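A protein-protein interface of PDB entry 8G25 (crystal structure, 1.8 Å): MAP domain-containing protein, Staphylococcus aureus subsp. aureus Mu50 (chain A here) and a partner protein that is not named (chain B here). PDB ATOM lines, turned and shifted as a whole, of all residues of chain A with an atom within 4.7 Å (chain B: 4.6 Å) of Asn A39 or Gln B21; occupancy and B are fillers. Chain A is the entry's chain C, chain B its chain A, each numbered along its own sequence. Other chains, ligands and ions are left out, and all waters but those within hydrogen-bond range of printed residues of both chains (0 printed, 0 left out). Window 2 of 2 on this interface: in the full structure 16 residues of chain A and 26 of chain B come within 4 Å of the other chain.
Asn A20 touches Gln B26. Tyr A37 touches Gly B25 (O to CA, 3.4 Å). Leu A38 touches Ala B24. Asn A39 touches Gln B21. Asn A39 touches Gly B25 (CG to N, 3.8 Å).
The backbone carbonyl oxygen of Gln B26 sits at hydrogen-bond distance from the backbone NH of Tyr A37, at 2.8 Å. O of Ala B24 lies within hydrogen-bond range of N of Asn A39, 3.1 Å away.
Printed residues of chain B within 4 Å of Tyr A37: Gly B25 (3.4 Å) and Gln B26 (2.8 Å). Of the printed residues of chain B, Leu A38 touches Ala B24. Printed residues of chain B within 4 Å of Asn A39: Gln B21, Ala B24 and Gly B25. Of chain A, only Asn A39 (3.8 Å) comes within 4 Å of Gln B21. Printed residues of chain A within 4 Å of Gln B26: Asn A20 and Tyr A37. The nearest residue of chain B that does not touch Asn A39 is Gln B26 (4.5 Å). The nearest printed residue of chain A that does not touch Gln B21 is Asn A20 (6.5 Å).
N of Ser B48 sits at hydrogen-bond distance from O of Gln B21. O of Gly B25 lies within hydrogen-bond range of NE2 of Gln B21. OD1 of Asn A20 lies close to OD1 of Asn A39 (2.7 Å). N of Gln B21 sits at hydrogen-bond distance from O of Asn B49 (2.9 Å).
Hydrophobic or aromatic side chains of chain A within 4 Å of the printed part of chain B: Tyr A37 and Leu A38. Printed residues of chain B that touch a printed residue of chain A: Gln B21, Ala B24, Gly B25 and Gln B26. Among the printed residues, 7 pairs touch across the chains.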
ATOM      1  N   MET A  18      19.496 -19.853  -6.155  1.00  0.00           N
ATOM      2  CA  MET A  18      20.801 -19.688  -5.530  1.00  0.00           C
ATOM      3  C   MET A  18      21.534 -18.492  -6.123  1.00  0.00           C
ATOM      4  O   MET A  18      21.492 -18.253  -7.333  1.00  0.00           O
ATOM      5  CB  MET A  18      21.664 -20.951  -5.687  1.00  0.00           C
ATOM      6  CG  MET A  18      21.108 -22.178  -4.976  1.00  0.00           C
ATOM      7  SD  MET A  18      21.334 -22.120  -3.187  1.00  0.00           S
ATOM      8  CE  MET A  18      20.033 -23.226  -2.648  1.00  0.00           C
ATOM      9  N   GLN A  19      22.186 -17.740  -5.247  1.00  0.00           N
ATOM     10  CA  GLN A  19      23.191 -16.768  -5.628  1.00  0.00           C
ATOM     11  C   GLN A  19      24.565 -17.426  -5.542  1.00  0.00           C
ATOM     12  O   GLN A  19      24.829 -18.228  -4.635  1.00  0.00           O
ATOM     13  CB  GLN A  19      23.108 -15.536  -4.720  1.00  0.00           C
ATOM     14  CG  GLN A  19      24.337 -14.628  -4.712  1.00  0.00           C
ATOM     15  CD  GLN A  19      24.508 -13.811  -5.988  1.00  0.00           C
ATOM     16  OE1 GLN A  19      23.916 -14.111  -7.025  1.00  0.00           O
ATOM     17  NE2 GLN A  19      25.329 -12.769  -5.910  1.00  0.00           N
ATOM     18  N   ASN A  20      25.426 -17.107  -6.509  1.00  0.00           N
ATOM     19  CA  ASN A  20      26.771 -17.670  -6.608  1.00  0.00           C
ATOM     20  C   ASN A  20      27.773 -16.579  -6.229  1.00  0.00           C
ATOM     21  O   ASN A  20      28.078 -15.691  -7.031  1.00  0.00           O
ATOM     22  CB  ASN A  20      27.033 -18.214  -8.015  1.00  0.00           C
ATOM     23  CG  ASN A  20      25.917 -19.128  -8.515  1.00  0.00           C
ATOM     24  OD1 ASN A  20      25.446 -20.014  -7.799  1.00  0.00           O
ATOM     25  ND2 ASN A  20      25.483 -18.904  -9.750  1.00  0.00           N
ATOM     26  N   TYR A  37      32.907 -20.436  -6.525  1.00  0.00           N
ATOM     27  CA  TYR A  37      31.711 -19.753  -6.059  1.00  0.00           C
ATOM     28  C   TYR A  37      31.059 -20.547  -4.938  1.00  0.00           C
ATOM     29  O   TYR A  37      30.987 -21.778  -4.988  1.00  0.00           O
ATOM     30  CB  TYR A  37      30.709 -19.557  -7.201  1.00  0.00           C
ATOM     31  CG  TYR A  37      31.282 -18.813  -8.386  1.00  0.00           C
ATOM     32  CD1 TYR A  37      32.017 -19.473  -9.367  1.00  0.00           C
ATOM     33  CD2 TYR A  37      31.099 -17.442  -8.517  1.00  0.00           C
ATOM     34  CE1 TYR A  37      32.551 -18.780 -10.451  1.00  0.00           C
ATOM     35  CE2 TYR A  37      31.620 -16.748  -9.589  1.00  0.00           C
ATOM     36  CZ  TYR A  37      32.342 -17.419 -10.552  1.00  0.00           C
ATOM     37  OH  TYR A  37      32.860 -16.714 -11.615  1.00  0.00           O
ATOM     38  N   LEU A  38      30.585 -19.833  -3.929  1.00  0.00           N
ATOM     39  CA  LEU A  38      29.829 -20.400  -2.825  1.00  0.00           C
ATOM     40  C   LEU A  38      28.356 -20.131  -3.087  1.00  0.00           C
ATOM     41  O   LEU A  38      27.988 -19.010  -3.444  1.00  0.00           O
ATOM     42  CB  LEU A  38      30.258 -19.769  -1.501  1.00  0.00           C
ATOM     43  CG  LEU A  38      29.422 -20.058  -0.258  1.00  0.00           C
ATOM     44  CD1 LEU A  38      29.582 -21.506   0.183  1.00  0.00           C
ATOM     45  CD2 LEU A  38      29.811 -19.103   0.863  1.00  0.00           C
ATOM     46  N   ASN A  39      27.520 -21.145  -2.930  1.00  0.00           N
ATOM     47  CA  ASN A  39      26.101 -21.001  -3.226  1.00  0.00           C
ATOM     48  C   ASN A  39      25.329 -20.649  -1.959  1.00  0.00           C
ATOM     49  O   ASN A  39      25.504 -21.294  -0.919  1.00  0.00           O
ATOM     50  CB  ASN A  39      25.547 -22.278  -3.856  1.00  0.00           C
ATOM     51  CG  ASN A  39      25.850 -22.375  -5.344  1.00  0.00           C
ATOM     52  OD1 ASN A  39      26.628 -21.588  -5.885  1.00  0.00           O
ATOM     53  ND2 ASN A  39      25.232 -23.337  -6.009  1.00  0.00           N
ATOM     54  N   LEU A  40      24.491 -19.620  -2.045  1.00  0.00           N
ATOM     55  CA  LEU A  40      23.586 -19.271  -0.959  1.00  0.00           C
ATOM     56  C   LEU A  40      22.168 -19.190  -1.497  1.00  0.00           C
ATOM     57  O   LEU A  40      21.966 -18.787  -2.642  1.00  0.00           O
ATOM     58  CB  LEU A  40      23.957 -17.925  -0.317  1.00  0.00           C
ATOM     59  CG  LEU A  40      25.390 -17.734   0.172  1.00  0.00           C
ATOM     60  CD1 LEU A  40      25.559 -16.323   0.710  1.00  0.00           C
ATOM     61  CD2 LEU A  40      25.735 -18.766   1.230  1.00  0.00           C
ATOM     62  N   PRO A  41      21.167 -19.572  -0.708  1.00  0.00           N
ATOM     63  CA  PRO A  41      19.786 -19.427  -1.183  1.00  0.00           C
ATOM     64  C   PRO A  41      19.509 -17.966  -1.492  1.00  0.00           C
ATOM     65  O   PRO A  41      19.823 -17.079  -0.697  1.00  0.00           O
ATOM     66  CB  PRO A  41      18.946 -19.942  -0.011  1.00  0.00           C
ATOM     67  CG  PRO A  41      19.880 -20.785   0.789  1.00  0.00           C
ATOM     68  CD  PRO A  41      21.221 -20.136   0.650  1.00  0.00           C
ATOM     69  N   GLN B  19      33.292 -26.971 -16.115  1.00  0.00           N
ATOM     70  CA  GLN B  19      32.288 -26.468 -15.188  1.00  0.00           C
ATOM     71  C   GLN B  19      32.085 -27.535 -14.127  1.00  0.00           C
ATOM     72  O   GLN B  19      31.646 -28.646 -14.439  1.00  0.00           O
ATOM     73  CB  GLN B  19      30.967 -26.152 -15.903  1.00  0.00           C
ATOM     74  CG  GLN B  19      31.060 -25.024 -16.911  1.00  0.00           C
ATOM     75  CD  GLN B  19      29.789 -24.832 -17.719  1.00  0.00           C
ATOM     76  OE1 GLN B  19      28.964 -23.970 -17.407  1.00  0.00           O
ATOM     77  NE2 GLN B  19      29.631 -25.625 -18.772  1.00  0.00           N
ATOM     78  N   ILE B  20      32.401 -27.203 -12.884  1.00  0.00           N
ATOM     79  CA  ILE B  20      32.447 -28.162 -11.792  1.00  0.00           C
ATOM     80  C   ILE B  20      31.364 -27.771 -10.803  1.00  0.00           C
ATOM     81  O   ILE B  20      31.303 -26.616 -10.379  1.00  0.00           O
ATOM     82  CB  ILE B  20      33.841 -28.170 -11.124  1.00  0.00           C
ATOM     83  CG1 ILE B  20      34.928 -28.527 -12.139  1.00  0.00           C
ATOM     84  CG2 ILE B  20      33.865 -29.120  -9.970  1.00  0.00           C
ATOM     85  CD1 ILE B  20      35.765 -27.341 -12.537  1.00  0.00           C
ATOM     86  N   GLN B  21      30.504 -28.713 -10.443  1.00  0.00           N
ATOM     87  CA  GLN B  21      29.420 -28.432  -9.511  1.00  0.00           C
ATOM     88  C   GLN B  21      29.477 -29.419  -8.354  1.00  0.00           C
ATOM     89  O   GLN B  21      29.696 -30.617  -8.560  1.00  0.00           O
ATOM     90  CB  GLN B  21      28.043 -28.508 -10.200  1.00  0.00           C
ATOM     91  CG  GLN B  21      26.840 -28.370  -9.257  1.00  0.00           C
ATOM     92  CD  GLN B  21      26.447 -26.924  -8.996  1.00  0.00           C
ATOM     93  OE1 GLN B  21      26.449 -26.096  -9.909  1.00  0.00           O
ATOM     94  NE2 GLN B  21      26.104 -26.614  -7.745  1.00  0.00           N
ATOM     95  N   SER B  22      29.294 -28.902  -7.146  1.00  0.00           N
ATOM     96  CA  SER B  22      29.173 -29.680  -5.925  1.00  0.00           C
ATOM     97  C   SER B  22      28.013 -29.096  -5.136  1.00  0.00           C
ATOM     98  O   SER B  22      27.569 -27.979  -5.424  1.00  0.00           O
ATOM     99  CB  SER B  22      30.469 -29.633  -5.103  1.00  0.00           C
ATOM    100  OG  SER B  22      31.557 -30.184  -5.831  1.00  0.00           O
ATOM    101  N   ALA B  24      25.972 -26.885  -3.043  1.00  0.00           N
ATOM    102  CA  ALA B  24      26.208 -25.513  -2.597  1.00  0.00           C
ATOM    103  C   ALA B  24      27.551 -24.947  -3.076  1.00  0.00           C
ATOM    104  O   ALA B  24      28.171 -24.141  -2.378  1.00  0.00           O
ATOM    105  CB  ALA B  24      26.104 -25.405  -1.071  1.00  0.00           C
ATOM    106  N   GLY B  25      28.016 -25.311  -4.270  1.00  0.00           N
ATOM    107  CA  GLY B  25      29.183 -24.633  -4.808  1.00  0.00           C
ATOM    108  C   GLY B  25      29.443 -24.976  -6.257  1.00  0.00           C
ATOM    109  O   GLY B  25      29.005 -26.014  -6.762  1.00  0.00           O
ATOM    110  N   GLN B  26      30.198 -24.096  -6.914  1.00  0.00           N
ATOM    111  CA  GLN B  26      30.607 -24.362  -8.285  1.00  0.00           C
ATOM    112  C   GLN B  26      31.996 -23.784  -8.532  1.00  0.00           C
ATOM    113  O   GLN B  26      32.476 -22.923  -7.795  1.00  0.00           O
ATOM    114  CB  GLN B  26      29.595 -23.804  -9.290  1.00  0.00           C
ATOM    115  CG  GLN B  26      29.523 -22.295  -9.349  1.00  0.00           C
ATOM    116  CD  GLN B  26      28.378 -21.811 -10.214  1.00  0.00           C
ATOM    117  OE1 GLN B  26      28.423 -20.712 -10.768  1.00  0.00           O
ATOM    118  NE2 GLN B  26      27.339 -22.629 -10.330  1.00  0.00           N
ATOM    119  N   GLY B  47      35.522 -31.876  -8.411  1.00  0.00           N
ATOM    120  CA  GLY B  47      34.233 -31.626  -7.790  1.00  0.00           C
ATOM    121  C   GLY B  47      33.302 -32.795  -8.046  1.00  0.00           C
ATOM    122  O   GLY B  47      33.678 -33.779  -8.685  1.00  0.00           O
ATOM    123  N   SER B  48      32.068 -32.683  -7.530  1.00  0.00           N
ATOM    124  CA  SER B  48      31.128 -33.812  -7.590  1.00  0.00           C
ATOM    125  C   SER B  48      30.728 -34.145  -9.019  1.00  0.00           C
ATOM    126  O   SER B  48      30.569 -35.322  -9.374  1.00  0.00           O
ATOM    127  CB  SER B  48      29.869 -33.513  -6.776  1.00  0.00           C
ATOM    128  OG  SER B  48      30.158 -33.370  -5.404  1.00  0.00           O
ATOM    129  N   ASN B  49      30.505 -33.126  -9.835  1.00  0.00           N
ATOM    130  CA  ASN B  49      30.095 -33.315 -11.214  1.00  0.00           C
ATOM    131  C   ASN B  49      30.905 -32.364 -12.066  1.00  0.00           C
ATOM    132  O   ASN B  49      31.123 -31.219 -11.671  1.00  0.00           O
ATOM    133  CB  ASN B  49      28.601 -33.051 -11.388  1.00  0.00           C
ATOM    134  CG  ASN B  49      27.758 -34.098 -10.713  1.00  0.00           C
ATOM    135  OD1 ASN B  49      27.613 -35.211 -11.220  1.00  0.00           O
ATOM    136  ND2 ASN B  49      27.209 -33.760  -9.555  1.00  0.00           N
